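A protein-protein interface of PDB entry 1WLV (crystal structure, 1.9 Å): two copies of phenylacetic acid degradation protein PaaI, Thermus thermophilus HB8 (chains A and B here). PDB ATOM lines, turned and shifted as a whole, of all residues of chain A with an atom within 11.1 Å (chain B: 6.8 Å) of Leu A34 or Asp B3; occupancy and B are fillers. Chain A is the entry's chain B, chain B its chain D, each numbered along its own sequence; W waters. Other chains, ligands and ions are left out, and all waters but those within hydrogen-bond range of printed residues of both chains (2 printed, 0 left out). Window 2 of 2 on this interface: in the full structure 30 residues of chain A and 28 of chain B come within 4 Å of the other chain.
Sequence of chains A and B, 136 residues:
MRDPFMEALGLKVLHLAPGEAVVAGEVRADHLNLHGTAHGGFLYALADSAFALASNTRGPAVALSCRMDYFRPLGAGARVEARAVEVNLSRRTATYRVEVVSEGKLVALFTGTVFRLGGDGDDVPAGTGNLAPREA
The backbone carbonyl oxygen (O) of Asp A30 lies close to the backbone NH (N) of Phe B5, 3.5 Å away. The backbone carbonyl oxygen of Leu A32 lies within hydrogen-bond range of the backbone NH of Phe B5 (3.1 Å). OD2 of Asp B3 sits at hydrogen-bond distance from N of Leu A34 (3.5 Å). A ring nitrogen (NE2) of His A39 lies within hydrogen-bond range of the side-chain hydroxyl of Ser B49, 3.2 Å away.
O of Leu A9 lies close to NE2 of His A31. The guanidinium group of Arg A28 is in salt-bridge range of the side-chain carboxylate of Asp A30 (2.9 Å). The side-chain amide oxygen (OD1) of Asn A33 sits at hydrogen-bond distance from the backbone NH (N) of His A35 (2.7 Å). ND2 of Asn A33 sits at hydrogen-bond distance from OG1 of Thr A37, at 3.0 Å. OD1 of Asp B3 sits at hydrogen-bond distance from N of Phe B5. The backbone carbonyl oxygen (O) of Ala B52 is in hydrogen-bond range of the side-chain amide nitrogen (ND2) of Asn B56 (2.7 Å).
Among the printed residues, merely in contact across the chains: Leu A9 with Phe B5 (3.6 Å), Ala A29 with Pro B4 (3.3 Å), Asp A30 with Pro B4 (3.7 Å), Asp A30 with Ala B8 (3.8 Å), His A31 with Phe B5 (3.9 Å), Leu A32 with Asp B3 (3.6 Å), Leu A32 with Pro B4 (3.4 Å), Asn A33 with Asp B3 (3.4 Å), Asn A33 with Pro B4 (3.8 Å), His A35 with Asn B56 (3.7 Å), His A39 with Asp B3 (3.5 Å), His A39 with Phe B5 (3.4 Å), Gly A41 with Phe B5 (3.8 Å) and Phe A42 with Phe B5 (3.7 Å).
Printed residues of chain B within 4 Å of Leu A9: Phe B5. Of the printed residues of chain B, Ala A29 touches Pro B4. Leu A34 touches one residue of chain B. Ala A38 touches none of the printed residues of chain B. Printed residues of chain B within 4 Å of His A39: Asp B3, Phe B5 and Ser B49. Of chain A, only Leu A32 (3.6 Å), Asn A33 (3.4 Å), Leu A34 (3.1 Å) and His A39 (3.5 Å) come within 4 Å of Asp B3. Pro B4 touches four residues of chain A. No residue of chain A comes within 4 Å of Met B6. Glu B7 touches none of the printed residues of chain A. The nearest residue of chain A that does not touch Asp B3 is His A35 (6.1 Å).
Of the 18 printed residues of chain A, 11 touch a printed residue of chain B. Hydrophobic or aromatic side chains of chain A that line the printed part of chain B: Leu A9, Leu A34, His A35 and His A39. Of the 10 printed residues of chain B, 6 touch a printed residue of chain A. Printed residues of chain B that touch a printed residue of chain A: Asp B3, Pro B4, Phe B5, Ala B8, Ser B49 and Asn B56. Hydrophobic or aromatic side chains of chain B within 4 Å of the printed part of chain A: Pro B4, Phe B5 and Ala B8. Among the printed residues, 18 pairs touch across the chains. Among the printed residues, no Asp or Glu carboxylate lies within 4 Å of a Lys or Arg side-chain nitrogen of the other chain.
No position is printed for both chains.
Water W1 lies within hydrogen-bond range of the side-chain carboxylate (OD2) of Asp B3 (2.8 Å), a ring nitrogen (NE2) of His A39 (2.8 Å) and the side-chain sulfur (SD) of Met B6 (3.4 Å). Water W2 lies within hydrogen-bond range of NE2 of His A35 and ND2 of Asn B56.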
ATOM      1  N   LEU A   9      -7.766   8.776  22.802  1.00  0.00           N
ATOM      2  CA  LEU A   9      -8.581   9.693  23.594  1.00  0.00           C
ATOM      3  C   LEU A   9      -7.841  10.967  23.978  1.00  0.00           C
ATOM      4  O   LEU A   9      -8.397  11.828  24.663  1.00  0.00           O
ATOM      5  CB  LEU A   9      -9.087   8.999  24.863  1.00  0.00           C
ATOM      6  CG  LEU A   9      -9.995   7.776  24.694  1.00  0.00           C
ATOM      7  CD1 LEU A   9     -10.478   7.305  26.068  1.00  0.00           C
ATOM      8  CD2 LEU A   9     -11.172   8.126  23.812  1.00  0.00           C
ATOM      9  N   VAL A  27     -11.660  17.303  27.643  1.00  0.00           N
ATOM     10  CA  VAL A  27     -12.874  16.798  27.027  1.00  0.00           C
ATOM     11  C   VAL A  27     -12.980  17.441  25.650  1.00  0.00           C
ATOM     12  O   VAL A  27     -13.028  18.663  25.534  1.00  0.00           O
ATOM     13  CB  VAL A  27     -14.122  17.158  27.867  1.00  0.00           C
ATOM     14  CG1 VAL A  27     -15.380  16.656  27.176  1.00  0.00           C
ATOM     15  CG2 VAL A  27     -13.999  16.545  29.263  1.00  0.00           C
ATOM     16  N   ARG A  28     -12.997  16.616  24.610  1.00  0.00           N
ATOM     17  CA  ARG A  28     -13.092  17.113  23.241  1.00  0.00           C
ATOM     18  C   ARG A  28     -14.484  16.849  22.688  1.00  0.00           C
ATOM     19  O   ARG A  28     -15.290  16.164  23.316  1.00  0.00           O
ATOM     20  CB  ARG A  28     -12.057  16.423  22.353  1.00  0.00           C
ATOM     21  CG  ARG A  28     -10.635  16.496  22.889  1.00  0.00           C
ATOM     22  CD  ARG A  28      -9.636  15.854  21.923  1.00  0.00           C
ATOM     23  NE  ARG A  28     -10.046  14.513  21.509  1.00  0.00           N
ATOM     24  CZ  ARG A  28      -9.201  13.511  21.279  1.00  0.00           C
ATOM     25  NH1 ARG A  28      -7.899  13.696  21.432  1.00  0.00           N
ATOM     26  NH2 ARG A  28      -9.660  12.326  20.890  1.00  0.00           N
ATOM     27  N   ALA A  29     -14.757  17.391  21.507  1.00  0.00           N
ATOM     28  CA  ALA A  29     -16.048  17.217  20.866  1.00  0.00           C
ATOM     29  C   ALA A  29     -16.390  15.740  20.684  1.00  0.00           C
ATOM     30  O   ALA A  29     -17.551  15.351  20.811  1.00  0.00           O
ATOM     31  CB  ALA A  29     -16.056  17.924  19.508  1.00  0.00           C
ATOM     32  N   ASP A  30     -15.381  14.921  20.395  1.00  0.00           N
ATOM     33  CA  ASP A  30     -15.609  13.494  20.175  1.00  0.00           C
ATOM     34  C   ASP A  30     -15.791  12.671  21.452  1.00  0.00           C
ATOM     35  O   ASP A  30     -15.982  11.457  21.392  1.00  0.00           O
ATOM     36  CB  ASP A  30     -14.479  12.898  19.315  1.00  0.00           C
ATOM     37  CG  ASP A  30     -13.097  13.050  19.948  1.00  0.00           C
ATOM     38  OD1 ASP A  30     -12.697  14.189  20.268  1.00  0.00           O
ATOM     39  OD2 ASP A  30     -12.401  12.024  20.111  1.00  0.00           O
ATOM     40  N   HIS A  31     -15.750  13.337  22.601  1.00  0.00           N
ATOM     41  CA  HIS A  31     -15.903  12.671  23.893  1.00  0.00           C
ATOM     42  C   HIS A  31     -17.273  12.935  24.505  1.00  0.00           C
ATOM     43  O   HIS A  31     -17.589  12.431  25.580  1.00  0.00           O
ATOM     44  CB  HIS A  31     -14.820  13.161  24.856  1.00  0.00           C
ATOM     45  CG  HIS A  31     -13.430  12.843  24.402  1.00  0.00           C
ATOM     46  ND1 HIS A  31     -12.346  13.641  24.701  1.00  0.00           N
ATOM     47  CD2 HIS A  31     -12.943  11.799  23.692  1.00  0.00           C
ATOM     48  CE1 HIS A  31     -11.252  13.101  24.193  1.00  0.00           C
ATOM     49  NE2 HIS A  31     -11.588  11.982  23.576  1.00  0.00           N
ATOM     50  N   LEU A  32     -18.089  13.721  23.814  1.00  0.00           N
ATOM     51  CA  LEU A  32     -19.408  14.063  24.334  1.00  0.00           C
ATOM     52  C   LEU A  32     -20.468  13.002  24.071  1.00  0.00           C
ATOM     53  O   LEU A  32     -20.320  12.160  23.186  1.00  0.00           O
ATOM     54  CB  LEU A  32     -19.876  15.391  23.733  1.00  0.00           C
ATOM     55  CG  LEU A  32     -18.954  16.606  23.880  1.00  0.00           C
ATOM     56  CD1 LEU A  32     -19.602  17.810  23.190  1.00  0.00           C
ATOM     57  CD2 LEU A  32     -18.700  16.905  25.359  1.00  0.00           C
ATOM     58  N   ASN A  33     -21.531  13.046  24.865  1.00  0.00           N
ATOM     59  CA  ASN A  33     -22.657  12.140  24.697  1.00  0.00           C
ATOM     60  C   ASN A  33     -23.718  12.968  23.977  1.00  0.00           C
ATOM     61  O   ASN A  33     -23.479  14.129  23.653  1.00  0.00           O
ATOM     62  CB  ASN A  33     -23.190  11.668  26.054  1.00  0.00           C
ATOM     63  CG  ASN A  33     -23.453  12.814  27.011  1.00  0.00           C
ATOM     64  OD1 ASN A  33     -24.006  13.841  26.628  1.00  0.00           O
ATOM     65  ND2 ASN A  33     -23.067  12.636  28.272  1.00  0.00           N
ATOM     66  N   LEU A  34     -24.884  12.383  23.731  1.00  0.00           N
ATOM     67  CA  LEU A  34     -25.955  13.100  23.049  1.00  0.00           C
ATOM     68  C   LEU A  34     -26.392  14.364  23.783  1.00  0.00           C
ATOM     69  O   LEU A  34     -26.871  15.313  23.161  1.00  0.00           O
ATOM     70  CB  LEU A  34     -27.165  12.182  22.856  1.00  0.00           C
ATOM     71  CG  LEU A  34     -27.043  11.140  21.744  1.00  0.00           C
ATOM     72  CD1 LEU A  34     -28.218  10.173  21.802  1.00  0.00           C
ATOM     73  CD2 LEU A  34     -26.989  11.854  20.398  1.00  0.00           C
ATOM     74  N   HIS A  35     -26.214  14.382  25.101  1.00  0.00           N
ATOM     75  CA  HIS A  35     -26.620  15.524  25.916  1.00  0.00           C
ATOM     76  C   HIS A  35     -25.631  16.688  25.930  1.00  0.00           C
ATOM     77  O   HIS A  35     -25.872  17.701  26.582  1.00  0.00           O
ATOM     78  CB  HIS A  35     -26.892  15.064  27.350  1.00  0.00           C
ATOM     79  CG  HIS A  35     -27.807  13.882  27.435  1.00  0.00           C
ATOM     80  ND1 HIS A  35     -29.041  13.849  26.819  1.00  0.00           N
ATOM     81  CD2 HIS A  35     -27.663  12.684  28.051  1.00  0.00           C
ATOM     82  CE1 HIS A  35     -29.617  12.683  27.052  1.00  0.00           C
ATOM     83  NE2 HIS A  35     -28.801  11.958  27.797  1.00  0.00           N
ATOM     84  N   GLY A  36     -24.516  16.546  25.222  1.00  0.00           N
ATOM     85  CA  GLY A  36     -23.541  17.621  25.176  1.00  0.00           C
ATOM     86  C   GLY A  36     -22.524  17.651  26.302  1.00  0.00           C
ATOM     87  O   GLY A  36     -21.759  18.611  26.416  1.00  0.00           O
ATOM     88  N   THR A  37     -22.507  16.622  27.146  1.00  0.00           N
ATOM     89  CA  THR A  37     -21.536  16.570  28.239  1.00  0.00           C
ATOM     90  C   THR A  37     -20.621  15.363  28.047  1.00  0.00           C
ATOM     91  O   THR A  37     -20.916  14.478  27.244  1.00  0.00           O
ATOM     92  CB  THR A  37     -22.220  16.468  29.626  1.00  0.00           C
ATOM     93  OG1 THR A  37     -23.037  15.294  29.679  1.00  0.00           O
ATOM     94  CG2 THR A  37     -23.084  17.695  29.888  1.00  0.00           C
ATOM     95  N   ALA A  38     -19.507  15.337  28.775  1.00  0.00           N
ATOM     96  CA  ALA A  38     -18.555  14.235  28.675  1.00  0.00           C
ATOM     97  C   ALA A  38     -19.244  12.890  28.885  1.00  0.00           C
ATOM     98  O   ALA A  38     -19.941  12.685  29.876  1.00  0.00           O
ATOM     99  CB  ALA A  38     -17.441  14.412  29.700  1.00  0.00           C
ATOM    100  N   HIS A  39     -19.037  11.982  27.938  1.00  0.00           N
ATOM    101  CA  HIS A  39     -19.619  10.648  27.978  1.00  0.00           C
ATOM    102  C   HIS A  39     -19.064   9.893  29.191  1.00  0.00           C
ATOM    103  O   HIS A  39     -17.887  10.017  29.521  1.00  0.00           O
ATOM    104  CB  HIS A  39     -19.267   9.927  26.674  1.00  0.00           C
ATOM    105  CG  HIS A  39     -20.007   8.645  26.455  1.00  0.00           C
ATOM    106  ND1 HIS A  39     -19.752   7.502  27.181  1.00  0.00           N
ATOM    107  CD2 HIS A  39     -20.956   8.311  25.549  1.00  0.00           C
ATOM    108  CE1 HIS A  39     -20.508   6.517  26.729  1.00  0.00           C
ATOM    109  NE2 HIS A  39     -21.247   6.981  25.739  1.00  0.00           N
ATOM    110  N   GLY A  40     -19.918   9.126  29.860  1.00  0.00           N
ATOM    111  CA  GLY A  40     -19.473   8.377  31.024  1.00  0.00           C
ATOM    112  C   GLY A  40     -18.336   7.426  30.701  1.00  0.00           C
ATOM    113  O   GLY A  40     -17.533   7.086  31.571  1.00  0.00           O
ATOM    114  N   GLY A  41     -18.272   6.991  29.445  1.00  0.00           N
ATOM    115  CA  GLY A  41     -17.224   6.080  29.023  1.00  0.00           C
ATOM    116  C   GLY A  41     -15.875   6.769  28.944  1.00  0.00           C
ATOM    117  O   GLY A  41     -14.839   6.143  29.176  1.00  0.00           O
ATOM    118  N   PHE A  42     -15.885   8.056  28.606  1.00  0.00           N
ATOM    119  CA  PHE A  42     -14.644   8.821  28.519  1.00  0.00           C
ATOM    120  C   PHE A  42     -14.040   9.004  29.910  1.00  0.00           C
ATOM    121  O   PHE A  42     -12.854   8.753  30.116  1.00  0.00           O
ATOM    122  CB  PHE A  42     -14.886  10.204  27.898  1.00  0.00           C
ATOM    123  CG  PHE A  42     -13.682  11.108  27.961  1.00  0.00           C
ATOM    124  CD1 PHE A  42     -12.552  10.842  27.189  1.00  0.00           C
ATOM    125  CD2 PHE A  42     -13.655  12.189  28.836  1.00  0.00           C
ATOM    126  CE1 PHE A  42     -11.407  11.646  27.295  1.00  0.00           C
ATOM    127  CE2 PHE A  42     -12.518  12.993  28.949  1.00  0.00           C
ATOM    128  CZ  PHE A  42     -11.395  12.719  28.178  1.00  0.00           C
ATOM    129  N   LEU A  74     -19.293  17.380  32.847  1.00  0.00           N
ATOM    130  CA  LEU A  74     -18.266  18.251  32.290  1.00  0.00           C
ATOM    131  C   LEU A  74     -18.592  18.562  30.843  1.00  0.00           C
ATOM    132  O   LEU A  74     -19.159  17.730  30.135  1.00  0.00           O
ATOM    133  CB  LEU A  74     -16.892  17.587  32.359  1.00  0.00           C
ATOM    134  CG  LEU A  74     -16.264  17.411  33.743  1.00  0.00           C
ATOM    135  CD1 LEU A  74     -14.916  16.724  33.600  1.00  0.00           C
ATOM    136  CD2 LEU A  74     -16.114  18.771  34.414  1.00  0.00           C
ATOM    137  N   ASP B   3     -24.640  10.392  19.035  1.00  0.00           N
ATOM    138  CA  ASP B   3     -23.698  10.379  20.193  1.00  0.00           C
ATOM    139  C   ASP B   3     -22.260  10.411  19.676  1.00  0.00           C
ATOM    140  O   ASP B   3     -21.748   9.413  19.172  1.00  0.00           O
ATOM    141  CB  ASP B   3     -23.932   9.125  21.035  1.00  0.00           C
ATOM    142  CG  ASP B   3     -23.104   9.107  22.303  1.00  0.00           C
ATOM    143  OD1 ASP B   3     -21.862   9.066  22.207  1.00  0.00           O
ATOM    144  OD2 ASP B   3     -23.699   9.131  23.402  1.00  0.00           O
ATOM    145  N   PRO B   4     -21.591  11.568  19.797  1.00  0.00           N
ATOM    146  CA  PRO B   4     -20.209  11.752  19.340  1.00  0.00           C
ATOM    147  C   PRO B   4     -19.213  10.669  19.759  1.00  0.00           C
ATOM    148  O   PRO B   4     -18.445  10.177  18.934  1.00  0.00           O
ATOM    149  CB  PRO B   4     -19.847  13.124  19.905  1.00  0.00           C
ATOM    150  CG  PRO B   4     -21.146  13.856  19.808  1.00  0.00           C
ATOM    151  CD  PRO B   4     -22.122  12.825  20.352  1.00  0.00           C
ATOM    152  N   PHE B   5     -19.227  10.294  21.035  1.00  0.00           N
ATOM    153  CA  PHE B   5     -18.292   9.285  21.530  1.00  0.00           C
ATOM    154  C   PHE B   5     -18.561   7.908  20.930  1.00  0.00           C
ATOM    155  O   PHE B   5     -17.628   7.174  20.609  1.00  0.00           O
ATOM    156  CB  PHE B   5     -18.348   9.223  23.063  1.00  0.00           C
ATOM    157  CG  PHE B   5     -17.191   8.486  23.689  1.00  0.00           C
ATOM    158  CD1 PHE B   5     -15.877   8.844  23.394  1.00  0.00           C
ATOM    159  CD2 PHE B   5     -17.417   7.451  24.594  1.00  0.00           C
ATOM    160  CE1 PHE B   5     -14.805   8.181  23.993  1.00  0.00           C
ATOM    161  CE2 PHE B   5     -16.355   6.785  25.198  1.00  0.00           C
ATOM    162  CZ  PHE B   5     -15.045   7.149  24.899  1.00  0.00           C
ATOM    163  N   MET B   6     -19.833   7.549  20.782  1.00  0.00           N
ATOM    164  CA  MET B   6     -20.173   6.255  20.199  1.00  0.00           C
ATOM    165  C   MET B   6     -19.669   6.198  18.763  1.00  0.00           C
ATOM    166  O   MET B   6     -19.120   5.187  18.325  1.00  0.00           O
ATOM    167  CB  MET B   6     -21.686   6.027  20.224  1.00  0.00           C
ATOM    168  CG  MET B   6     -22.252   5.765  21.609  1.00  0.00           C
ATOM    169  SD  MET B   6     -24.031   5.410  21.579  1.00  0.00           S
ATOM    170  CE  MET B   6     -24.037   3.844  20.759  1.00  0.00           C
ATOM    171  N   GLU B   7     -19.861   7.292  18.031  1.00  0.00           N
ATOM    172  CA  GLU B   7     -19.410   7.365  16.646  1.00  0.00           C
ATOM    173  C   GLU B   7     -17.889   7.310  16.576  1.00  0.00           C
ATOM    174  O   GLU B   7     -17.317   6.645  15.712  1.00  0.00           O
ATOM    175  CB  GLU B   7     -19.919   8.653  15.995  1.00  0.00           C
ATOM    176  CG  GLU B   7     -21.429   8.703  15.856  1.00  0.00           C
ATOM    177  CD  GLU B   7     -21.914   9.982  15.204  1.00  0.00           C
ATOM    178  OE1 GLU B   7     -21.460  10.287  14.079  1.00  0.00           O
ATOM    179  OE2 GLU B   7     -22.751  10.682  15.813  1.00  0.00           O
ATOM    180  N   ALA B   8     -17.231   8.013  17.489  1.00  0.00           N
ATOM    181  CA  ALA B   8     -15.775   8.015  17.521  1.00  0.00           C
ATOM    182  C   ALA B   8     -15.257   6.595  17.739  1.00  0.00           C
ATOM    183  O   ALA B   8     -14.246   6.206  17.156  1.00  0.00           O
ATOM    184  CB  ALA B   8     -15.271   8.932  18.638  1.00  0.00           C
ATOM    185  N   SER B  49     -22.644   2.698  26.953  1.00  0.00           N
ATOM    186  CA  SER B  49     -23.461   3.253  25.877  1.00  0.00           C
ATOM    187  C   SER B  49     -24.813   2.537  25.785  1.00  0.00           C
ATOM    188  O   SER B  49     -25.848   3.178  25.596  1.00  0.00           O
ATOM    189  CB  SER B  49     -22.724   3.152  24.540  1.00  0.00           C
ATOM    190  OG  SER B  49     -21.584   3.991  24.529  1.00  0.00           O
ATOM    191  N   ALA B  52     -26.747   3.731  28.727  1.00  0.00           N
ATOM    192  CA  ALA B  52     -27.293   5.071  28.510  1.00  0.00           C
ATOM    193  C   ALA B  52     -28.520   5.054  27.597  1.00  0.00           C
ATOM    194  O   ALA B  52     -29.523   5.718  27.872  1.00  0.00           O
ATOM    195  CB  ALA B  52     -26.219   5.987  27.914  1.00  0.00           C
ATOM    196  N   LEU B  53     -28.437   4.300  26.508  1.00  0.00           N
ATOM    197  CA  LEU B  53     -29.547   4.220  25.564  1.00  0.00           C
ATOM    198  C   LEU B  53     -30.765   3.557  26.197  1.00  0.00           C
ATOM    199  O   LEU B  53     -31.883   4.058  26.084  1.00  0.00           O
ATOM    200  CB  LEU B  53     -29.120   3.450  24.317  1.00  0.00           C
ATOM    201  CG  LEU B  53     -28.144   4.197  23.402  1.00  0.00           C
ATOM    202  CD1 LEU B  53     -27.597   3.259  22.344  1.00  0.00           C
ATOM    203  CD2 LEU B  53     -28.862   5.371  22.759  1.00  0.00           C
ATOM    204  N   ASN B  56     -32.380   5.888  28.830  1.00  0.00           N
ATOM    205  CA  ASN B  56     -33.028   7.073  28.285  1.00  0.00           C
ATOM    206  C   ASN B  56     -34.347   6.779  27.571  1.00  0.00           C
ATOM    207  O   ASN B  56     -35.088   7.701  27.237  1.00  0.00           O
ATOM    208  CB  ASN B  56     -32.066   7.834  27.368  1.00  0.00           C
ATOM    209  CG  ASN B  56     -31.074   8.684  28.149  1.00  0.00           C
ATOM    210  OD1 ASN B  56     -31.461   9.610  28.869  1.00  0.00           O
ATOM    211  ND2 ASN B  56     -29.791   8.374  28.014  1.00  0.00           N
HETATM  212  O   HOH W   1     -23.905   6.684  24.770  1.00  0.00           O
HETATM  213  O   HOH W   2     -27.009  10.019  26.751  1.00  0.00           O
